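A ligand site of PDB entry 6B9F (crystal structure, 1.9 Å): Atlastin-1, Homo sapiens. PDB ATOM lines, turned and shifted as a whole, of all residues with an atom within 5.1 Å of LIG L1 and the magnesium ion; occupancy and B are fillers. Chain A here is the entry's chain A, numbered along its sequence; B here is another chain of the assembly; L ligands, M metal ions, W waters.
Water W4 lies within hydrogen-bond range of the side-chain carboxylate (OD1) of Asp 146 (2.6 Å) and the backbone carbonyl oxygen (O) of Thr 147 (2.8 Å). Water W2 bridges O6 of LIG L1 (2.7 Å) and O of Ser 111 (2.9 Å). Water W3 lies within hydrogen-bond range of an oxygen (O11) of LIG L1 (2.7 Å), the backbone carbonyl oxygen (O) of Pro 270 (2.7 Å) and the backbone NH (N) of Asp 218 (3.0 Å). Water W7 lies within hydrogen-bond range of O of Ala 277 (2.7 Å) and O9 of LIG L1 (2.7 Å). Water W5 bridges the backbone carbonyl oxygen (O) of Lys 78 and a nitrogen (N3) of LIG L1.
The side-chain hydroxyl (OG) of Ser 81 lies close to the side-chain carboxylate (OD2) of Asp 146 (2.5 Å). OG of Ser 81 lies close to O of Ser 111 (3.5 Å). O of Ala 75 lies within hydrogen-bond range of NZ of Lys 80 (3.0 Å). The backbone carbonyl oxygen (O) of Leu 269 lies within hydrogen-bond range of the backbone NH (N) of Asp 218. NH2 of Arg 217 is in hydrogen-bond range of O of Gly 79 (3.1 Å). The guanidinium group of Arg 77 sits at hydrogen-bond distance from the backbone carbonyl oxygen of Arg 113 (2.7 Å). NZ of Lys 78 sits close to NE2 of Gln 180 of chain B, at 3.2 Å. The side-chain carboxylate (OE2) of Glu 119 lies within salt-bridge range of the guanidinium group (NE) of Arg 113.
N of Ser 81 is in hydrogen-bond range of O5 of LIG L1, 3.2 Å away. The backbone NH (N) of Lys 80 lies within hydrogen-bond range of an oxygen (O2) of LIG L1, at 2.8 Å. O2 of LIG L1 lies within salt-bridge range of NZ of Lys 80. The side-chain carboxylate (OD1) of Asp 218 is in hydrogen-bond range of a nitrogen (N3) of LIG L1, at 2.7 Å. An oxygen (O5) of LIG L1 lies within hydrogen-bond range of the backbone NH (N) of Phe 82, at 2.8 Å. N2 of LIG L1 sits at hydrogen-bond distance from NH2 of Arg 217 (2.8 Å). The backbone NH (N) of Gly 79 sits at hydrogen-bond distance from an oxygen (O4) of LIG L1 (2.9 Å). N of Arg 77 sits close to O3 of LIG L1 (3.3 Å). The guanidinium group of Arg 77 lies within salt-bridge range of an oxygen (O6) of LIG L1, 3.0 Å away. O of Val 276 sits at hydrogen-bond distance from O10 of LIG L1 (3.1 Å). The backbone NH (N) of Lys 78 is in hydrogen-bond range of an oxygen (O2) of LIG L1 (3.1 Å). The backbone NH of Arg 113 sits at hydrogen-bond distance from an oxygen (O6) of LIG L1. An oxygen (O9) of LIG L1 lies close to the backbone NH of Gly 114 (3.5 Å). The backbone NH of Thr 120 sits at hydrogen-bond distance from a fluorine (F1) of LG2 L2 (2.9 Å). NZ of Lys 80 sits at hydrogen-bond distance from F2 of LG2 L2 (2.6 Å). The backbone NH (N) of Arg 77 sits at hydrogen-bond distance from a fluorine (F4) of LG2 L2 (2.9 Å). A fluorine (F4) of LG2 L2 lies within hydrogen-bond range of the guanidinium group of Arg 77 (2.8 Å). A fluorine (F1) of LG2 L2 lies within hydrogen-bond range of the backbone NH (N) of Glu 119 (2.5 Å).
An oxygen (O3) of LIG L1 is bound to an aluminium atom (AL1) of LG2 L2, 2.0 Å away.
The magnesium ion is bound by O1 of LIG L1 (2.0 Å), water W4 (2.0 Å), F3 of LG2 L2 (2.0 Å), OG of Ser 81 (2.1 Å), OG1 of Thr 120 (2.1 Å) and water W2 (2.4 Å).
Residues that only touch LIG L1: Trp 112 (3.3 Å), Pro 272 (3.3 Å), Phe 282 (3.7 Å), His 271 (3.7 Å), Phe 293 (3.9 Å) and Ala 277 (3.9 Å). 17 residues have an atom within 4 Å of LIG L1: Arg 77, Lys 78, Gly 79, Lys 80, Ser 81, Phe 82, Trp 112, Arg 113, Gly 114, Arg 217, Asp 218, His 271, Pro 272, Val 276, Ala 277, Phe 282 and Phe 293.
Asp 146 touches the magnesium ion (OD2 to MG, 3.9 Å). Three residues have an atom within 4 Å of the magnesium ion: Ser 81, Thr 120 and Asp 146.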
ATOM      1  N   ALA A  75      24.729 -27.451 -12.087  1.00  0.00           N
ATOM      2  CA  ALA A  75      25.254 -26.930 -10.838  1.00  0.00           C
ATOM      3  C   ALA A  75      24.315 -27.242  -9.670  1.00  0.00           C
ATOM      4  O   ALA A  75      23.100 -27.331  -9.825  1.00  0.00           O
ATOM      5  CB  ALA A  75      25.446 -25.414 -10.930  1.00  0.00           C
ATOM      6  N   PHE A  76      24.901 -27.371  -8.483  1.00  0.00           N
ATOM      7  CA  PHE A  76      24.107 -27.764  -7.325  1.00  0.00           C
ATOM      8  C   PHE A  76      23.267 -26.587  -6.782  1.00  0.00           C
ATOM      9  O   PHE A  76      23.569 -25.415  -6.998  1.00  0.00           O
ATOM     10  CB  PHE A  76      25.043 -28.350  -6.238  1.00  0.00           C
ATOM     11  CG  PHE A  76      25.702 -27.321  -5.324  1.00  0.00           C
ATOM     12  CD1 PHE A  76      26.572 -26.357  -5.817  1.00  0.00           C
ATOM     13  CD2 PHE A  76      25.499 -27.376  -3.958  1.00  0.00           C
ATOM     14  CE1 PHE A  76      27.173 -25.425  -4.963  1.00  0.00           C
ATOM     15  CE2 PHE A  76      26.105 -26.451  -3.097  1.00  0.00           C
ATOM     16  CZ  PHE A  76      26.943 -25.478  -3.604  1.00  0.00           C
ATOM     17  N   ARG A  77      22.189 -26.944  -6.072  1.00  0.00           N
ATOM     18  CA  ARG A  77      21.287 -25.991  -5.394  1.00  0.00           C
ATOM     19  C   ARG A  77      20.500 -25.115  -6.370  1.00  0.00           C
ATOM     20  O   ARG A  77      20.230 -23.945  -6.068  1.00  0.00           O
ATOM     21  CB  ARG A  77      22.037 -25.083  -4.401  1.00  0.00           C
ATOM     22  CG  ARG A  77      22.811 -25.758  -3.269  1.00  0.00           C
ATOM     23  CD  ARG A  77      21.951 -26.333  -2.175  1.00  0.00           C
ATOM     24  NE  ARG A  77      21.172 -27.484  -2.604  1.00  0.00           N
ATOM     25  CZ  ARG A  77      19.939 -27.697  -2.176  1.00  0.00           C
ATOM     26  NH1 ARG A  77      19.373 -26.831  -1.334  1.00  0.00           N
ATOM     27  NH2 ARG A  77      19.269 -28.753  -2.594  1.00  0.00           N
ATOM     28  N   LYS A  78      20.086 -25.650  -7.522  1.00  0.00           N
ATOM     29  CA  LYS A  78      19.440 -24.851  -8.572  1.00  0.00           C
ATOM     30  C   LYS A  78      18.046 -25.362  -8.929  1.00  0.00           C
ATOM     31  O   LYS A  78      17.517 -24.978  -9.979  1.00  0.00           O
ATOM     32  CB  LYS A  78      20.280 -24.833  -9.848  1.00  0.00           C
ATOM     33  CG  LYS A  78      21.657 -24.210  -9.720  1.00  0.00           C
ATOM     34  CD  LYS A  78      21.625 -22.815  -9.107  1.00  0.00           C
ATOM     35  CE  LYS A  78      22.981 -22.130  -9.333  1.00  0.00           C
ATOM     36  NZ  LYS A  78      23.319 -21.149  -8.254  1.00  0.00           N
ATOM     37  N   GLY A  79      17.448 -26.203  -8.097  1.00  0.00           N
ATOM     38  CA  GLY A  79      16.083 -26.648  -8.332  1.00  0.00           C
ATOM     39  C   GLY A  79      15.911 -27.842  -9.239  1.00  0.00           C
ATOM     40  O   GLY A  79      14.847 -27.998  -9.842  1.00  0.00           O
ATOM     41  N   LYS A  80      16.928 -28.715  -9.341  1.00  0.00           N
ATOM     42  CA  LYS A  80      16.829 -29.844 -10.275  1.00  0.00           C
ATOM     43  C   LYS A  80      15.817 -30.884  -9.777  1.00  0.00           C
ATOM     44  O   LYS A  80      14.967 -31.355 -10.547  1.00  0.00           O
ATOM     45  CB  LYS A  80      18.203 -30.490 -10.458  1.00  0.00           C
ATOM     46  CG  LYS A  80      19.225 -29.592 -11.129  1.00  0.00           C
ATOM     47  CD  LYS A  80      20.515 -30.365 -11.418  1.00  0.00           C
ATOM     48  CE  LYS A  80      21.174 -30.803 -10.104  1.00  0.00           C
ATOM     49  NZ  LYS A  80      21.397 -29.674  -9.141  1.00  0.00           N
ATOM     50  N   SER A  81      15.928 -31.277  -8.501  1.00  0.00           N
ATOM     51  CA  SER A  81      15.014 -32.265  -7.941  1.00  0.00           C
ATOM     52  C   SER A  81      13.593 -31.700  -7.899  1.00  0.00           C
ATOM     53  O   SER A  81      12.623 -32.417  -8.150  1.00  0.00           O
ATOM     54  CB  SER A  81      15.468 -32.670  -6.526  1.00  0.00           C
ATOM     55  OG  SER A  81      16.774 -33.247  -6.513  1.00  0.00           O
ATOM     56  N   PHE A  82      13.467 -30.409  -7.570  1.00  0.00           N
ATOM     57  CA  PHE A  82      12.198 -29.698  -7.640  1.00  0.00           C
ATOM     58  C   PHE A  82      11.524 -29.883  -9.004  1.00  0.00           C
ATOM     59  O   PHE A  82      10.369 -30.294  -9.089  1.00  0.00           O
ATOM     60  CB  PHE A  82      12.469 -28.211  -7.338  1.00  0.00           C
ATOM     61  CG  PHE A  82      11.244 -27.328  -7.230  1.00  0.00           C
ATOM     62  CD1 PHE A  82      10.573 -27.199  -6.025  1.00  0.00           C
ATOM     63  CD2 PHE A  82      10.846 -26.547  -8.295  1.00  0.00           C
ATOM     64  CE1 PHE A  82       9.465 -26.344  -5.896  1.00  0.00           C
ATOM     65  CE2 PHE A  82       9.753 -25.686  -8.190  1.00  0.00           C
ATOM     66  CZ  PHE A  82       9.056 -25.590  -6.982  1.00  0.00           C
ATOM     67  N   SER A 111      13.900 -35.951  -3.170  1.00  0.00           N
ATOM     68  CA  SER A 111      14.069 -35.004  -2.084  1.00  0.00           C
ATOM     69  C   SER A 111      14.616 -33.661  -2.591  1.00  0.00           C
ATOM     70  O   SER A 111      15.667 -33.601  -3.229  1.00  0.00           O
ATOM     71  CB  SER A 111      15.000 -35.588  -1.025  1.00  0.00           C
ATOM     72  OG  SER A 111      15.239 -34.625  -0.019  1.00  0.00           O
ATOM     73  N   TRP A 112      13.901 -32.584  -2.295  1.00  0.00           N
ATOM     74  CA  TRP A 112      14.343 -31.231  -2.624  1.00  0.00           C
ATOM     75  C   TRP A 112      14.156 -30.371  -1.368  1.00  0.00           C
ATOM     76  O   TRP A 112      13.310 -30.660  -0.525  1.00  0.00           O
ATOM     77  CB  TRP A 112      13.537 -30.673  -3.808  1.00  0.00           C
ATOM     78  CG  TRP A 112      12.099 -30.430  -3.466  1.00  0.00           C
ATOM     79  CD1 TRP A 112      11.067 -31.321  -3.541  1.00  0.00           C
ATOM     80  CD2 TRP A 112      11.547 -29.205  -2.950  1.00  0.00           C
ATOM     81  NE1 TRP A 112       9.889 -30.726  -3.117  1.00  0.00           N
ATOM     82  CE2 TRP A 112      10.168 -29.436  -2.729  1.00  0.00           C
ATOM     83  CE3 TRP A 112      12.085 -27.953  -2.646  1.00  0.00           C
ATOM     84  CZ2 TRP A 112       9.318 -28.447  -2.234  1.00  0.00           C
ATOM     85  CZ3 TRP A 112      11.221 -26.962  -2.156  1.00  0.00           C
ATOM     86  CH2 TRP A 112       9.867 -27.217  -1.950  1.00  0.00           C
ATOM     87  N   ARG A 113      14.954 -29.302  -1.247  1.00  0.00           N
ATOM     88  CA  ARG A 113      14.832 -28.394  -0.119  1.00  0.00           C
ATOM     89  C   ARG A 113      15.741 -27.204  -0.349  1.00  0.00           C
ATOM     90  O   ARG A 113      16.665 -27.264  -1.171  1.00  0.00           O
ATOM     91  CB  ARG A 113      15.193 -29.059   1.204  1.00  0.00           C
ATOM     92  CG  ARG A 113      16.553 -29.718   1.162  1.00  0.00           C
ATOM     93  CD  ARG A 113      17.252 -29.629   2.535  1.00  0.00           C
ATOM     94  NE  ARG A 113      18.479 -30.417   2.499  1.00  0.00           N
ATOM     95  CZ  ARG A 113      19.686 -29.932   2.213  1.00  0.00           C
ATOM     96  NH1 ARG A 113      19.841 -28.640   1.931  1.00  0.00           N
ATOM     97  NH2 ARG A 113      20.748 -30.755   2.199  1.00  0.00           N
ATOM     98  N   GLY A 114      15.485 -26.131   0.415  1.00  0.00           N
ATOM     99  CA  GLY A 114      16.370 -24.986   0.492  1.00  0.00           C
ATOM    100  C   GLY A 114      17.593 -25.301   1.329  1.00  0.00           C
ATOM    101  O   GLY A 114      17.876 -26.450   1.681  1.00  0.00           O
ATOM    102  N   GLU A 119      21.808 -31.528  -1.282  1.00  0.00           N
ATOM    103  CA  GLU A 119      20.905 -32.586  -0.833  1.00  0.00           C
ATOM    104  C   GLU A 119      21.082 -33.870  -1.645  1.00  0.00           C
ATOM    105  O   GLU A 119      21.522 -34.887  -1.087  1.00  0.00           O
ATOM    106  CB  GLU A 119      19.448 -32.078  -0.859  1.00  0.00           C
ATOM    107  CG  GLU A 119      18.385 -33.164  -0.600  1.00  0.00           C
ATOM    108  CD  GLU A 119      18.446 -33.764   0.804  1.00  0.00           C
ATOM    109  OE1 GLU A 119      17.992 -34.911   0.991  1.00  0.00           O
ATOM    110  OE2 GLU A 119      18.946 -33.084   1.743  1.00  0.00           O
ATOM    111  N   THR A 120      20.794 -33.850  -2.945  1.00  0.00           N
ATOM    112  CA  THR A 120      20.966 -35.053  -3.765  1.00  0.00           C
ATOM    113  C   THR A 120      22.437 -35.436  -3.819  1.00  0.00           C
ATOM    114  O   THR A 120      23.300 -34.583  -4.079  1.00  0.00           O
ATOM    115  CB  THR A 120      20.456 -34.834  -5.203  1.00  0.00           C
ATOM    116  OG1 THR A 120      19.149 -34.247  -5.185  1.00  0.00           O
ATOM    117  CG2 THR A 120      20.391 -36.155  -5.962  1.00  0.00           C
ATOM    118  N   ASP A 146      17.600 -38.403 -11.444  1.00  0.00           N
ATOM    119  CA  ASP A 146      17.949 -37.171 -10.742  1.00  0.00           C
ATOM    120  C   ASP A 146      19.372 -37.292 -10.235  1.00  0.00           C
ATOM    121  O   ASP A 146      19.773 -38.374  -9.789  1.00  0.00           O
ATOM    122  CB  ASP A 146      16.959 -36.922  -9.571  1.00  0.00           C
ATOM    123  CG  ASP A 146      17.142 -35.565  -8.894  1.00  0.00           C
ATOM    124  OD1 ASP A 146      17.676 -34.615  -9.507  1.00  0.00           O
ATOM    125  OD2 ASP A 146      16.726 -35.454  -7.728  1.00  0.00           O
ATOM    126  N   THR A 147      20.142 -36.211 -10.289  1.00  0.00           N
ATOM    127  CA  THR A 147      21.582 -36.298 -10.096  1.00  0.00           C
ATOM    128  C   THR A 147      22.080 -35.287  -9.074  1.00  0.00           C
ATOM    129  O   THR A 147      21.482 -34.239  -8.829  1.00  0.00           O
ATOM    130  CB  THR A 147      22.365 -36.070 -11.416  1.00  0.00           C
ATOM    131  OG1 THR A 147      22.190 -34.710 -11.835  1.00  0.00           O
ATOM    132  CG2 THR A 147      21.910 -37.027 -12.539  1.00  0.00           C
ATOM    133  N   ARG A 217      17.066 -21.405 -15.845  1.00  0.00           N
ATOM    134  CA  ARG A 217      16.229 -20.980 -14.733  1.00  0.00           C
ATOM    135  C   ARG A 217      16.418 -19.489 -14.477  1.00  0.00           C
ATOM    136  O   ARG A 217      17.468 -18.923 -14.757  1.00  0.00           O
ATOM    137  CB  ARG A 217      16.565 -21.773 -13.465  1.00  0.00           C
ATOM    138  CG  ARG A 217      16.604 -23.290 -13.674  1.00  0.00           C
ATOM    139  CD  ARG A 217      15.199 -23.877 -13.896  1.00  0.00           C
ATOM    140  NE  ARG A 217      14.443 -24.079 -12.660  1.00  0.00           N
ATOM    141  CZ  ARG A 217      14.392 -25.232 -11.991  1.00  0.00           C
ATOM    142  NH1 ARG A 217      15.060 -26.279 -12.441  1.00  0.00           N
ATOM    143  NH2 ARG A 217      13.644 -25.358 -10.904  1.00  0.00           N
ATOM    144  N   ASP A 218      15.363 -18.865 -13.933  1.00  0.00           N
ATOM    145  CA  ASP A 218      15.399 -17.451 -13.539  1.00  0.00           C
ATOM    146  C   ASP A 218      15.842 -16.556 -14.702  1.00  0.00           C
ATOM    147  O   ASP A 218      16.584 -15.591 -14.525  1.00  0.00           O
ATOM    148  CB  ASP A 218      16.309 -17.213 -12.326  1.00  0.00           C
ATOM    149  CG  ASP A 218      15.909 -18.027 -11.109  1.00  0.00           C
ATOM    150  OD1 ASP A 218      14.820 -18.647 -11.085  1.00  0.00           O
ATOM    151  OD2 ASP A 218      16.693 -18.043 -10.148  1.00  0.00           O
ATOM    152  N   LEU A 269      13.045 -20.132 -18.636  1.00  0.00           N
ATOM    153  CA  LEU A 269      12.046 -20.252 -17.600  1.00  0.00           C
ATOM    154  C   LEU A 269      12.058 -19.024 -16.668  1.00  0.00           C
ATOM    155  O   LEU A 269      13.146 -18.580 -16.253  1.00  0.00           O
ATOM    156  CB  LEU A 269      12.291 -21.534 -16.799  1.00  0.00           C
ATOM    157  CG  LEU A 269      11.158 -22.177 -15.995  1.00  0.00           C
ATOM    158  CD1 LEU A 269       9.971 -22.563 -16.878  1.00  0.00           C
ATOM    159  CD2 LEU A 269      11.668 -23.391 -15.213  1.00  0.00           C
ATOM    160  N   PRO A 270      10.898 -18.466 -16.337  1.00  0.00           N
ATOM    161  CA  PRO A 270      10.855 -17.338 -15.400  1.00  0.00           C
ATOM    162  C   PRO A 270      11.267 -17.756 -13.998  1.00  0.00           C
ATOM    163  O   PRO A 270      11.222 -18.928 -13.623  1.00  0.00           O
ATOM    164  CB  PRO A 270       9.394 -16.882 -15.429  1.00  0.00           C
ATOM    165  CG  PRO A 270       8.751 -17.605 -16.644  1.00  0.00           C
ATOM    166  CD  PRO A 270       9.551 -18.870 -16.792  1.00  0.00           C
ATOM    167  N   HIS A 271      11.697 -16.766 -13.224  1.00  0.00           N
ATOM    168  CA  HIS A 271      11.907 -16.967 -11.795  1.00  0.00           C
ATOM    169  C   HIS A 271      10.580 -17.383 -11.142  1.00  0.00           C
ATOM    170  O   HIS A 271       9.527 -16.853 -11.493  1.00  0.00           O
ATOM    171  CB  HIS A 271      12.427 -15.667 -11.171  1.00  0.00           C
ATOM    172  CG  HIS A 271      12.996 -15.807  -9.785  1.00  0.00           C
ATOM    173  ND1 HIS A 271      12.218 -16.065  -8.665  1.00  0.00           N
ATOM    174  CD2 HIS A 271      14.260 -15.629  -9.321  1.00  0.00           C
ATOM    175  CE1 HIS A 271      12.989 -16.104  -7.594  1.00  0.00           C
ATOM    176  NE2 HIS A 271      14.229 -15.825  -7.954  1.00  0.00           N
ATOM    177  N   PRO A 272      10.594 -18.330 -10.204  1.00  0.00           N
ATOM    178  CA  PRO A 272       9.317 -18.764  -9.600  1.00  0.00           C
ATOM    179  C   PRO A 272       8.847 -17.900  -8.438  1.00  0.00           C
ATOM    180  O   PRO A 272       7.829 -18.227  -7.820  1.00  0.00           O
ATOM    181  CB  PRO A 272       9.649 -20.185  -9.127  1.00  0.00           C
ATOM    182  CG  PRO A 272      11.107 -20.103  -8.773  1.00  0.00           C
ATOM    183  CD  PRO A 272      11.723 -19.144  -9.753  1.00  0.00           C
ATOM    184  N   VAL A 276       9.501 -18.997  -3.235  1.00  0.00           N
ATOM    185  CA  VAL A 276      10.098 -20.274  -3.620  1.00  0.00           C
ATOM    186  C   VAL A 276      11.586 -20.286  -3.295  1.00  0.00           C
ATOM    187  O   VAL A 276      12.100 -21.272  -2.752  1.00  0.00           O
ATOM    188  CB  VAL A 276       9.856 -20.537  -5.112  1.00  0.00           C
ATOM    189  CG1 VAL A 276      10.710 -21.736  -5.587  1.00  0.00           C
ATOM    190  CG2 VAL A 276       8.367 -20.781  -5.340  1.00  0.00           C
ATOM    191  N   ALA A 277      12.297 -19.209  -3.619  1.00  0.00           N
ATOM    192  CA  ALA A 277      13.733 -19.182  -3.381  1.00  0.00           C
ATOM    193  C   ALA A 277      14.103 -18.993  -1.895  1.00  0.00           C
ATOM    194  O   ALA A 277      15.140 -19.532  -1.468  1.00  0.00           O
ATOM    195  CB  ALA A 277      14.379 -18.077  -4.219  1.00  0.00           C
ATOM    196  N   PHE A 282       8.246 -22.980   2.674  1.00  0.00           N
ATOM    197  CA  PHE A 282       7.752 -23.378   1.361  1.00  0.00           C
ATOM    198  C   PHE A 282       7.918 -24.887   1.153  1.00  0.00           C
ATOM    199  O   PHE A 282       9.011 -25.447   1.362  1.00  0.00           O
ATOM    200  CB  PHE A 282       8.487 -22.580   0.284  1.00  0.00           C
ATOM    201  CG  PHE A 282       8.186 -23.028  -1.121  1.00  0.00           C
ATOM    202  CD1 PHE A 282       6.945 -22.778  -1.697  1.00  0.00           C
ATOM    203  CD2 PHE A 282       9.156 -23.711  -1.868  1.00  0.00           C
ATOM    204  CE1 PHE A 282       6.673 -23.201  -2.989  1.00  0.00           C
ATOM    205  CE2 PHE A 282       8.884 -24.133  -3.161  1.00  0.00           C
ATOM    206  CZ  PHE A 282       7.649 -23.872  -3.730  1.00  0.00           C
ATOM    207  N   PHE A 293       5.644 -18.307 -13.921  1.00  0.00           N
ATOM    208  CA  PHE A 293       6.447 -19.528 -13.840  1.00  0.00           C
ATOM    209  C   PHE A 293       5.570 -20.757 -14.093  1.00  0.00           C
ATOM    210  O   PHE A 293       5.930 -21.627 -14.895  1.00  0.00           O
ATOM    211  CB  PHE A 293       7.114 -19.616 -12.465  1.00  0.00           C
ATOM    212  CG  PHE A 293       7.918 -20.879 -12.257  1.00  0.00           C
ATOM    213  CD1 PHE A 293       7.324 -22.033 -11.754  1.00  0.00           C
ATOM    214  CD2 PHE A 293       9.272 -20.902 -12.571  1.00  0.00           C
ATOM    215  CE1 PHE A 293       8.068 -23.203 -11.561  1.00  0.00           C
ATOM    216  CE2 PHE A 293      10.034 -22.080 -12.368  1.00  0.00           C
ATOM    217  CZ  PHE A 293       9.435 -23.227 -11.871  1.00  0.00           C
ATOM    218  N   GLN B 180      24.305 -15.927  -5.839  1.00  0.00           N
ATOM    219  CA  GLN B 180      23.556 -16.900  -5.040  1.00  0.00           C
ATOM    220  C   GLN B 180      24.381 -17.765  -4.086  1.00  0.00           C
ATOM    221  O   GLN B 180      23.877 -18.157  -3.032  1.00  0.00           O
ATOM    222  CB  GLN B 180      22.752 -17.843  -5.936  1.00  0.00           C
ATOM    223  CG  GLN B 180      21.574 -17.189  -6.671  1.00  0.00           C
ATOM    224  CD  GLN B 180      20.818 -18.196  -7.524  1.00  0.00           C
ATOM    225  OE1 GLN B 180      20.207 -17.843  -8.536  1.00  0.00           O
ATOM    226  NE2 GLN B 180      20.844 -19.456  -7.121  1.00  0.00           N
ATOM    227  N   PHE B 221      19.175 -17.890   1.645  1.00  0.00           N
ATOM    228  CA  PHE B 221      18.992 -18.669   2.866  1.00  0.00           C
ATOM    229  C   PHE B 221      19.318 -17.866   4.123  1.00  0.00           C
ATOM    230  O   PHE B 221      20.192 -18.268   4.911  1.00  0.00           O
ATOM    231  CB  PHE B 221      19.829 -19.940   2.768  1.00  0.00           C
ATOM    232  CG  PHE B 221      19.705 -20.615   1.422  1.00  0.00           C
ATOM    233  CD1 PHE B 221      18.468 -21.057   0.984  1.00  0.00           C
ATOM    234  CD2 PHE B 221      20.809 -20.775   0.588  1.00  0.00           C
ATOM    235  CE1 PHE B 221      18.333 -21.684  -0.261  1.00  0.00           C
ATOM    236  CE2 PHE B 221      20.684 -21.379  -0.657  1.00  0.00           C
ATOM    237  CZ  PHE B 221      19.436 -21.834  -1.065  1.00  0.00           C
HETATM  238  P1  LIG L   1      18.886 -29.294  -6.576  1.00  0.00           P
HETATM  239  O1  LIG L   1      18.174 -30.589  -6.806  1.00  0.00           O
HETATM  240  O2  LIG L   1      19.342 -28.625  -7.854  1.00  0.00           O
HETATM  241  O3  LIG L   1      19.995 -29.360  -5.578  1.00  0.00           O
HETATM  242  O4  LIG L   1      17.865 -28.211  -5.977  1.00  0.00           O
HETATM  243  P2  LIG L   1      16.505 -28.498  -5.197  1.00  0.00           P
HETATM  244  O5  LIG L   1      15.534 -29.117  -6.154  1.00  0.00           O
HETATM  245  O6  LIG L   1      16.666 -29.323  -3.950  1.00  0.00           O
HETATM  246  O7  LIG L   1      16.033 -26.983  -4.882  1.00  0.00           O
HETATM  247  C1  LIG L   1      16.794 -26.098  -4.031  1.00  0.00           C
HETATM  248  C2  LIG L   1      16.078 -24.752  -3.868  1.00  0.00           C
HETATM  249  O8  LIG L   1      15.745 -24.134  -5.128  1.00  0.00           O
HETATM  250  C3  LIG L   1      14.739 -24.926  -3.172  1.00  0.00           C
HETATM  251  O9  LIG L   1      14.684 -23.912  -2.161  1.00  0.00           O
HETATM  252  C4  LIG L   1      13.709 -24.674  -4.277  1.00  0.00           C
HETATM  253  O10 LIG L   1      12.508 -24.129  -3.763  1.00  0.00           O
HETATM  254  C5  LIG L   1      14.415 -23.616  -5.081  1.00  0.00           C
HETATM  255  N1  LIG L   1      13.985 -23.498  -6.494  1.00  0.00           N
HETATM  256  C6  LIG L   1      13.336 -24.380  -7.246  1.00  0.00           C
HETATM  257  N2  LIG L   1      13.191 -23.909  -8.509  1.00  0.00           N
HETATM  258  C7  LIG L   1      13.775 -22.704  -8.569  1.00  0.00           C
HETATM  259  C8  LIG L   1      14.007 -21.683  -9.610  1.00  0.00           C
HETATM  260  O11 LIG L   1      13.570 -21.862 -10.774  1.00  0.00           O
HETATM  261  N3  LIG L   1      14.665 -20.570  -9.257  1.00  0.00           N
HETATM  262  C9  LIG L   1      15.129 -20.369  -8.003  1.00  0.00           C
HETATM  263  N4  LIG L   1      15.794 -19.208  -7.706  1.00  0.00           N
HETATM  264  N5  LIG L   1      14.966 -21.288  -7.015  1.00  0.00           N
HETATM  265  C10 LIG L   1      14.317 -22.455  -7.243  1.00  0.00           C
HETATM  266 AL1  LG2 L   2      21.540 -30.635  -5.149  1.00  0.00          AL
HETATM  267  F1  LG2 L   2      20.808 -30.999  -3.552  1.00  0.00           F
HETATM  268  F2  LG2 L   2      22.276 -30.317  -6.750  1.00  0.00           F
HETATM  269  F3  LG2 L   2      20.593 -31.917  -5.898  1.00  0.00           F
HETATM  270  F4  LG2 L   2      22.396 -29.259  -4.385  1.00  0.00           F
HETATM  271 MG    MG M   1      18.633 -32.398  -6.115  1.00  0.00          MG
HETATM  272  O   HOH W   1      17.482 -20.881  -4.808  1.00  0.00           O
HETATM  273  O   HOH W   2      17.743 -31.773  -4.030  1.00  0.00           O
HETATM  274  O   HOH W   3      13.216 -20.765 -13.186  1.00  0.00           O
HETATM  275  O   HOH W   4      19.133 -33.052  -7.952  1.00  0.00           O
HETATM  276  O   HOH W   5      17.534 -22.099  -9.631  1.00  0.00           O
HETATM  277  O   HOH W   6      17.616 -18.485  -5.534  1.00  0.00           O
HETATM  278  O   HOH W   7      16.163 -21.704  -2.709  1.00  0.00           O
